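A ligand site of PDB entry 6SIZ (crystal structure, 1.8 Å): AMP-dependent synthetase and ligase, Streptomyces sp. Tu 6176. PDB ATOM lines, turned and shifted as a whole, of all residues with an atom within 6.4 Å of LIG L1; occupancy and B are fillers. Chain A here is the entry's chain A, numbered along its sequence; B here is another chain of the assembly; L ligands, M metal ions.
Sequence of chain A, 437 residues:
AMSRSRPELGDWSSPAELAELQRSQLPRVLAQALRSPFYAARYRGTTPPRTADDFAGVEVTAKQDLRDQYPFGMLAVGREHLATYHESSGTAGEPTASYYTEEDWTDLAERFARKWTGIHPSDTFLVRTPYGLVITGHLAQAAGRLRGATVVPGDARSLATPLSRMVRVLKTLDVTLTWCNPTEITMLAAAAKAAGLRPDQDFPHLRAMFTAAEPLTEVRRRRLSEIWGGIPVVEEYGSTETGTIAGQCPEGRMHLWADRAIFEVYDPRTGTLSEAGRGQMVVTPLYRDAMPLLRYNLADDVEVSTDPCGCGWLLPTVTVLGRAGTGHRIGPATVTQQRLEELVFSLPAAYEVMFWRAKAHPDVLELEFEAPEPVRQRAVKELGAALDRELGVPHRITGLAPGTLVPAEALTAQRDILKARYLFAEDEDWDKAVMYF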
ATOM      1  N   SER A  89     -25.093 -28.753  12.464  1.00  0.00           N
ATOM      2  CA  SER A  89     -23.921 -28.343  13.263  1.00  0.00           C
ATOM      3  C   SER A  89     -24.407 -27.977  14.674  1.00  0.00           C
ATOM      4  O   SER A  89     -25.628 -28.084  14.929  1.00  0.00           O
ATOM      5  CB  SER A  89     -23.189 -27.232  12.570  1.00  0.00           C
ATOM      6  OG  SER A  89     -23.992 -26.066  12.536  1.00  0.00           O
ATOM      7  N   PHE A 112     -29.689 -22.750  -3.942  1.00  0.00           N
ATOM      8  CA  PHE A 112     -28.239 -22.498  -3.789  1.00  0.00           C
ATOM      9  C   PHE A 112     -27.705 -21.875  -5.085  1.00  0.00           C
ATOM     10  O   PHE A 112     -26.921 -20.905  -5.024  1.00  0.00           O
ATOM     11  CB  PHE A 112     -27.461 -23.759  -3.428  1.00  0.00           C
ATOM     12  CG  PHE A 112     -25.993 -23.501  -3.214  1.00  0.00           C
ATOM     13  CD1 PHE A 112     -25.137 -23.334  -4.293  1.00  0.00           C
ATOM     14  CD2 PHE A 112     -25.480 -23.332  -1.946  1.00  0.00           C
ATOM     15  CE1 PHE A 112     -23.788 -23.089  -4.095  1.00  0.00           C
ATOM     16  CE2 PHE A 112     -24.134 -23.080  -1.733  1.00  0.00           C
ATOM     17  CZ  PHE A 112     -23.304 -22.939  -2.818  1.00  0.00           C
ATOM     18  N   VAL A 134     -23.425 -33.017   7.892  1.00  0.00           N
ATOM     19  CA  VAL A 134     -23.966 -31.662   7.582  1.00  0.00           C
ATOM     20  C   VAL A 134     -24.269 -31.575   6.090  1.00  0.00           C
ATOM     21  O   VAL A 134     -23.658 -32.319   5.293  1.00  0.00           O
ATOM     22  CB  VAL A 134     -23.046 -30.502   8.038  1.00  0.00           C
ATOM     23  CG1 VAL A 134     -22.783 -30.545   9.537  1.00  0.00           C
ATOM     24  CG2 VAL A 134     -21.745 -30.455   7.276  1.00  0.00           C
ATOM     25  N   ILE A 135     -25.220 -30.721   5.713  1.00  0.00           N
ATOM     26  CA  ILE A 135     -25.742 -30.689   4.321  1.00  0.00           C
ATOM     27  C   ILE A 135     -24.868 -29.827   3.405  1.00  0.00           C
ATOM     28  O   ILE A 135     -24.967 -29.992   2.172  1.00  0.00           O
ATOM     29  CB  ILE A 135     -27.203 -30.187   4.361  1.00  0.00           C
ATOM     30  CG1 ILE A 135     -27.989 -30.651   3.141  1.00  0.00           C
ATOM     31  CG2 ILE A 135     -27.252 -28.666   4.546  1.00  0.00           C
ATOM     32  CD1 ILE A 135     -29.466 -30.441   3.258  1.00  0.00           C
ATOM     33  N   THR A 136     -24.056 -28.939   3.999  1.00  0.00           N
ATOM     34  CA  THR A 136     -23.393 -27.801   3.322  1.00  0.00           C
ATOM     35  C   THR A 136     -22.635 -28.245   2.071  1.00  0.00           C
ATOM     36  O   THR A 136     -22.850 -27.672   1.018  1.00  0.00           O
ATOM     37  CB  THR A 136     -22.445 -27.078   4.285  1.00  0.00           C
ATOM     38  OG1 THR A 136     -23.038 -27.035   5.581  1.00  0.00           O
ATOM     39  CG2 THR A 136     -22.113 -25.684   3.807  1.00  0.00           C
ATOM     40  N   LEU A 139     -24.864 -29.800  -0.624  1.00  0.00           N
ATOM     41  CA  LEU A 139     -25.750 -28.780  -1.248  1.00  0.00           C
ATOM     42  C   LEU A 139     -24.974 -28.071  -2.363  1.00  0.00           C
ATOM     43  O   LEU A 139     -25.495 -27.994  -3.472  1.00  0.00           O
ATOM     44  CB  LEU A 139     -26.218 -27.804  -0.162  1.00  0.00           C
ATOM     45  CG  LEU A 139     -27.069 -26.632  -0.649  1.00  0.00           C
ATOM     46  CD1 LEU A 139     -28.314 -27.107  -1.386  1.00  0.00           C
ATOM     47  CD2 LEU A 139     -27.448 -25.760   0.539  1.00  0.00           C
ATOM     48  N   TRP A 179     -16.608 -22.196  -2.308  1.00  0.00           N
ATOM     49  CA  TRP A 179     -17.674 -22.213  -1.284  1.00  0.00           C
ATOM     50  C   TRP A 179     -17.046 -22.596   0.046  1.00  0.00           C
ATOM     51  O   TRP A 179     -16.470 -23.692   0.182  1.00  0.00           O
ATOM     52  CB  TRP A 179     -18.789 -23.194  -1.694  1.00  0.00           C
ATOM     53  CG  TRP A 179     -19.790 -23.583  -0.651  1.00  0.00           C
ATOM     54  CD1 TRP A 179     -19.955 -24.837  -0.157  1.00  0.00           C
ATOM     55  CD2 TRP A 179     -20.782 -22.769  -0.011  1.00  0.00           C
ATOM     56  NE1 TRP A 179     -20.995 -24.871   0.736  1.00  0.00           N
ATOM     57  CE2 TRP A 179     -21.518 -23.615   0.845  1.00  0.00           C
ATOM     58  CE3 TRP A 179     -21.127 -21.408  -0.070  1.00  0.00           C
ATOM     59  CZ2 TRP A 179     -22.580 -23.160   1.617  1.00  0.00           C
ATOM     60  CZ3 TRP A 179     -22.185 -20.960   0.687  1.00  0.00           C
ATOM     61  CH2 TRP A 179     -22.897 -21.826   1.525  1.00  0.00           C
ATOM     62  N   THR A 211     -20.072 -17.640   0.126  1.00  0.00           N
ATOM     63  CA  THR A 211     -19.891 -17.770   1.595  1.00  0.00           C
ATOM     64  C   THR A 211     -21.220 -17.717   2.339  1.00  0.00           C
ATOM     65  O   THR A 211     -22.216 -17.235   1.795  1.00  0.00           O
ATOM     66  CB  THR A 211     -18.879 -16.736   2.112  1.00  0.00           C
ATOM     67  OG1 THR A 211     -18.432 -17.199   3.392  1.00  0.00           O
ATOM     68  CG2 THR A 211     -19.450 -15.353   2.231  1.00  0.00           C
ATOM     69  N   ALA A 212     -21.206 -18.256   3.551  1.00  0.00           N
ATOM     70  CA  ALA A 212     -22.364 -18.340   4.452  1.00  0.00           C
ATOM     71  C   ALA A 212     -21.882 -18.833   5.810  1.00  0.00           C
ATOM     72  O   ALA A 212     -20.649 -19.056   5.950  1.00  0.00           O
ATOM     73  CB  ALA A 212     -23.392 -19.287   3.875  1.00  0.00           C
ATOM     74  N   ALA A 213     -22.806 -19.061   6.723  1.00  0.00           N
ATOM     75  CA  ALA A 213     -22.651 -19.871   7.967  1.00  0.00           C
ATOM     76  C   ALA A 213     -22.074 -19.039   9.121  1.00  0.00           C
ATOM     77  O   ALA A 213     -21.790 -19.641  10.179  1.00  0.00           O
ATOM     78  CB  ALA A 213     -21.790 -21.076   7.704  1.00  0.00           C
ATOM     79  N   GLU A 214     -21.827 -17.746   8.938  1.00  0.00           N
ATOM     80  CA  GLU A 214     -21.573 -16.830  10.082  1.00  0.00           C
ATOM     81  C   GLU A 214     -22.053 -15.423   9.780  1.00  0.00           C
ATOM     82  O   GLU A 214     -22.112 -14.976   8.644  1.00  0.00           O
ATOM     83  CB  GLU A 214     -20.137 -16.862  10.620  1.00  0.00           C
ATOM     84  CG  GLU A 214     -19.016 -16.908   9.622  1.00  0.00           C
ATOM     85  CD  GLU A 214     -17.611 -16.889  10.233  1.00  0.00           C
ATOM     86  OE1 GLU A 214     -16.820 -17.797   9.922  1.00  0.00           O
ATOM     87  OE2 GLU A 214     -17.249 -15.853  10.825  1.00  0.00           O
ATOM     88  N   GLU A 236     -24.778 -16.113   1.081  1.00  0.00           N
ATOM     89  CA  GLU A 236     -26.152 -16.661   1.223  1.00  0.00           C
ATOM     90  C   GLU A 236     -26.369 -16.970   2.704  1.00  0.00           C
ATOM     91  O   GLU A 236     -25.424 -16.939   3.487  1.00  0.00           O
ATOM     92  CB  GLU A 236     -26.399 -17.859   0.297  1.00  0.00           C
ATOM     93  CG  GLU A 236     -25.749 -19.152   0.742  1.00  0.00           C
ATOM     94  CD  GLU A 236     -26.336 -20.404   0.130  1.00  0.00           C
ATOM     95  OE1 GLU A 236     -26.277 -20.534  -1.122  1.00  0.00           O
ATOM     96  OE2 GLU A 236     -26.888 -21.231   0.883  1.00  0.00           O
ATOM     97  N   TYR A 237     -27.617 -17.252   3.028  1.00  0.00           N
ATOM     98  CA  TYR A 237     -28.151 -17.546   4.377  1.00  0.00           C
ATOM     99  C   TYR A 237     -28.998 -18.803   4.247  1.00  0.00           C
ATOM    100  O   TYR A 237     -29.842 -18.838   3.326  1.00  0.00           O
ATOM    101  CB  TYR A 237     -28.887 -16.329   4.904  1.00  0.00           C
ATOM    102  CG  TYR A 237     -29.701 -16.530   6.169  1.00  0.00           C
ATOM    103  CD1 TYR A 237     -29.236 -17.309   7.222  1.00  0.00           C
ATOM    104  CD2 TYR A 237     -30.925 -15.897   6.326  1.00  0.00           C
ATOM    105  CE1 TYR A 237     -29.988 -17.464   8.380  1.00  0.00           C
ATOM    106  CE2 TYR A 237     -31.673 -16.050   7.472  1.00  0.00           C
ATOM    107  CZ  TYR A 237     -31.205 -16.836   8.509  1.00  0.00           C
ATOM    108  OH  TYR A 237     -31.956 -16.987   9.646  1.00  0.00           O
ATOM    109  N   GLY A 238     -28.718 -19.818   5.062  1.00  0.00           N
ATOM    110  CA  GLY A 238     -29.427 -21.114   5.039  1.00  0.00           C
ATOM    111  C   GLY A 238     -29.344 -21.849   6.360  1.00  0.00           C
ATOM    112  O   GLY A 238     -28.706 -21.337   7.287  1.00  0.00           O
ATOM    113  N   SER A 239     -30.005 -23.005   6.430  1.00  0.00           N
ATOM    114  CA  SER A 239     -29.904 -23.977   7.544  1.00  0.00           C
ATOM    115  C   SER A 239     -30.076 -25.392   6.979  1.00  0.00           C
ATOM    116  O   SER A 239     -30.584 -25.537   5.839  1.00  0.00           O
ATOM    117  CB  SER A 239     -30.910 -23.686   8.632  1.00  0.00           C
ATOM    118  OG  SER A 239     -32.228 -24.061   8.250  1.00  0.00           O
ATOM    119  N   THR A 240     -29.645 -26.394   7.740  1.00  0.00           N
ATOM    120  CA  THR A 240     -29.816 -27.822   7.386  1.00  0.00           C
ATOM    121  C   THR A 240     -31.302 -28.147   7.208  1.00  0.00           C
ATOM    122  O   THR A 240     -31.643 -28.945   6.295  1.00  0.00           O
ATOM    123  CB  THR A 240     -29.158 -28.706   8.435  1.00  0.00           C
ATOM    124  OG1 THR A 240     -27.908 -28.099   8.729  1.00  0.00           O
ATOM    125  CG2 THR A 240     -29.002 -30.128   7.954  1.00  0.00           C
ATOM    126  N   GLY A 243     -32.621 -25.494   3.906  1.00  0.00           N
ATOM    127  CA  GLY A 243     -31.798 -25.136   2.723  1.00  0.00           C
ATOM    128  C   GLY A 243     -31.568 -23.639   2.658  1.00  0.00           C
ATOM    129  O   GLY A 243     -31.747 -22.956   3.693  1.00  0.00           O
ATOM    130  N   THR A 244     -31.137 -23.136   1.503  1.00  0.00           N
ATOM    131  CA  THR A 244     -30.785 -21.703   1.275  1.00  0.00           C
ATOM    132  C   THR A 244     -32.058 -20.860   1.294  1.00  0.00           C
ATOM    133  O   THR A 244     -32.913 -21.112   0.434  1.00  0.00           O
ATOM    134  CB  THR A 244     -30.096 -21.492  -0.066  1.00  0.00           C
ATOM    135  OG1 THR A 244     -29.008 -22.412  -0.099  1.00  0.00           O
ATOM    136  CG2 THR A 244     -29.602 -20.071  -0.273  1.00  0.00           C
ATOM    137  N   ILE A 245     -32.185 -19.913   2.215  1.00  0.00           N
ATOM    138  CA  ILE A 245     -33.427 -19.094   2.327  1.00  0.00           C
ATOM    139  C   ILE A 245     -33.166 -17.657   1.836  1.00  0.00           C
ATOM    140  O   ILE A 245     -34.167 -16.975   1.574  1.00  0.00           O
ATOM    141  CB  ILE A 245     -34.037 -19.174   3.734  1.00  0.00           C
ATOM    142  CG1 ILE A 245     -33.074 -18.749   4.838  1.00  0.00           C
ATOM    143  CG2 ILE A 245     -34.597 -20.576   3.987  1.00  0.00           C
ATOM    144  CD1 ILE A 245     -33.631 -18.904   6.224  1.00  0.00           C
ATOM    145  N   ALA A 246     -31.928 -17.232   1.623  1.00  0.00           N
ATOM    146  CA  ALA A 246     -31.637 -15.881   1.084  1.00  0.00           C
ATOM    147  C   ALA A 246     -30.295 -15.858   0.365  1.00  0.00           C
ATOM    148  O   ALA A 246     -29.371 -16.565   0.793  1.00  0.00           O
ATOM    149  CB  ALA A 246     -31.691 -14.835   2.178  1.00  0.00           C
ATOM    150  N   LYS B 419     -18.642 -23.312  15.028  1.00  0.00           N
ATOM    151  CA  LYS B 419     -18.375 -22.314  13.965  1.00  0.00           C
ATOM    152  C   LYS B 419     -17.546 -21.186  14.580  1.00  0.00           C
ATOM    153  O   LYS B 419     -17.591 -21.049  15.839  1.00  0.00           O
ATOM    154  CB  LYS B 419     -19.694 -21.796  13.388  1.00  0.00           C
ATOM    155  CG  LYS B 419     -20.589 -22.873  12.817  1.00  0.00           C
ATOM    156  CD  LYS B 419     -21.858 -22.313  12.205  1.00  0.00           C
ATOM    157  CE  LYS B 419     -23.014 -23.283  12.271  1.00  0.00           C
ATOM    158  NZ  LYS B 419     -24.308 -22.592  12.090  1.00  0.00           N
HETATM  159  O1  LIG L   1     -24.656 -23.588   7.443  1.00  0.00           O
HETATM  160  C1  LIG L   1     -25.639 -24.271   7.108  1.00  0.00           C
HETATM  161  O2  LIG L   1     -26.211 -25.071   7.888  1.00  0.00           O
HETATM  162  C2  LIG L   1     -26.200 -24.034   5.742  1.00  0.00           C
HETATM  163  C3  LIG L   1     -26.951 -24.990   5.045  1.00  0.00           C
HETATM  164  C4  LIG L   1     -27.469 -24.688   3.789  1.00  0.00           C
HETATM  165  C5  LIG L   1     -27.255 -23.455   3.165  1.00  0.00           C
HETATM  166  C6  LIG L   1     -26.512 -22.473   3.793  1.00  0.00           C
HETATM  167  O3  LIG L   1     -26.292 -21.257   3.251  1.00  0.00           O
HETATM  168  C7  LIG L   1     -25.954 -22.725   5.133  1.00  0.00           C
HETATM  169  N1  LIG L   1     -25.225 -21.777   5.781  1.00  0.00           N
HETATM  170  P1  LG2 L   2     -28.802 -25.807  15.970  1.00  0.00           P
HETATM  171  O1  LG2 L   2     -30.055 -25.817  15.121  1.00  0.00           O
HETATM  172  O2  LG2 L   2     -28.799 -27.037  16.846  1.00  0.00           O
HETATM  173  O3  LG2 L   2     -28.782 -24.558  16.834  1.00  0.00           O
HETATM  174  P2  LG2 L   2     -27.204 -24.617  13.875  1.00  0.00           P
HETATM  175  O4  LG2 L   2     -28.020 -23.376  14.184  1.00  0.00           O
HETATM  176  O5  LG2 L   2     -25.723 -24.487  13.653  1.00  0.00           O
HETATM  177  N1  LG2 L   2     -27.516 -25.791  14.969  1.00  0.00           N
HETATM  178  P3  LG2 L   2     -27.235 -25.382  11.013  1.00  0.00           P
HETATM  179  O6  LG2 L   2     -28.426 -25.698  10.168  1.00  0.00           O
HETATM  180  O7  LG2 L   2     -26.100 -26.349  11.082  1.00  0.00           O
HETATM  181  O8  LG2 L   2     -27.824 -25.182  12.496  1.00  0.00           O
HETATM  182  O9  LG2 L   2     -26.666 -23.919  10.659  1.00  0.00           O
HETATM  183  C1  LG2 L   2     -27.532 -22.878  10.122  1.00  0.00           C
HETATM  184  C2  LG2 L   2     -27.319 -21.579  10.875  1.00  0.00           C
HETATM  185  O10 LG2 L   2     -26.068 -20.955  10.492  1.00  0.00           O
HETATM  186  C3  LG2 L   2     -28.355 -20.491  10.611  1.00  0.00           C
HETATM  187  O11 LG2 L   2     -29.566 -20.691  11.313  1.00  0.00           O
HETATM  188  C4  LG2 L   2     -27.604 -19.276  11.149  1.00  0.00           C
HETATM  189  O12 LG2 L   2     -27.548 -19.254  12.557  1.00  0.00           O
HETATM  190  C5  LG2 L   2     -26.220 -19.546  10.583  1.00  0.00           C
HETATM  191  N2  LG2 L   2     -26.050 -18.915   9.264  1.00  0.00           N
HETATM  192  C6  LG2 L   2     -25.991 -19.509   8.015  1.00  0.00           C
HETATM  193  N3  LG2 L   2     -25.760 -18.639   7.049  1.00  0.00           N
HETATM  194  C7  LG2 L   2     -25.627 -17.413   7.707  1.00  0.00           C
HETATM  195  C8  LG2 L   2     -25.356 -16.102   7.269  1.00  0.00           C
HETATM  196  N4  LG2 L   2     -25.144 -15.772   5.988  1.00  0.00           N
HETATM  197  N5  LG2 L   2     -25.254 -15.124   8.204  1.00  0.00           N
HETATM  198  C9  LG2 L   2     -25.465 -15.444   9.488  1.00  0.00           C
HETATM  199  N6  LG2 L   2     -25.722 -16.633  10.019  1.00  0.00           N
HETATM  200  C10 LG2 L   2     -25.784 -17.582   9.073  1.00  0.00           C
HETATM  201 MG    MG M   1     -29.927 -26.108  12.662  1.00  0.00          MG
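The side-chain carboxylate (OE2) of Glu 236 lies within hydrogen-bond range of an oxygen (O3) of LIG L1, at 2.4 Å.
The backbone NH (N) of Gly 238 lies within hydrogen-bond range of an oxygen (O3) of LIG L1, at 3.4 Å.
The backbone carbonyl oxygen (O) of Glu 236 is in hydrogen-bond range of a nitrogen (N4) of LG2 L2 (2.8 Å).
An oxygen (O6) of LG2 L2 is in hydrogen-bond range of the backbone NH (N) of Thr 240 (2.8 Å).
An oxygen (O6) of LG2 L2 sits at hydrogen-bond distance from the side-chain hydroxyl (OG1) of Thr 240 (2.8 Å).
N of Ala 213 lies within hydrogen-bond range of N3 of LG2 L2, 3.0 Å away.
NZ of Lys 419 of chain B is in salt-bridge range of O5 of LG2 L2 (2.8 Å).
N of Ser 89 is in hydrogen-bond range of O7 of LG2 L2, 3.0 Å away.
A nitrogen (N1) of LG2 L2 lies within hydrogen-bond range of the backbone carbonyl oxygen (O) of Ser 89 (3.0 Å).
The side-chain hydroxyl of Ser 89 is in hydrogen-bond range of an oxygen (O7) of LG2 L2 (2.6 Å).
A nitrogen (N1) of LIG L1 sits close to a nitrogen (N3) of LG2 L2, 3.4 Å away.
OE2 of Glu 236 lies within hydrogen-bond range of OG1 of Thr 244 (2.6 Å).
N of Glu 236 lies within hydrogen-bond range of O of Thr 211 (2.9 Å).
The backbone NH (N) of Tyr 237 sits at hydrogen-bond distance from the backbone carbonyl oxygen (O) of Ala 246 (2.9 Å).
The backbone carbonyl oxygen (O) of Tyr 237 lies within hydrogen-bond range of the backbone NH (N) of Ile 245 (2.8 Å).
The backbone carbonyl oxygen (O) of Thr 136 sits close to the indole nitrogen (NE1) of Trp 179, 3.4 Å away.
Merely in contact with LIG L1: Leu 139, Ala 212, Thr 240, Ser 239, Ile 135, Ala 213, Tyr 237, Thr 244 and Trp 179.
Within 4 Å of LIG L1: Ile 135, Leu 139, Trp 179, Ala 212, Ala 213, Glu 236, Tyr 237, Gly 238, Ser 239, Thr 240 and Thr 244.
Along chain A the residues within 4 Å of LIG L1 span positions 135 to 244.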
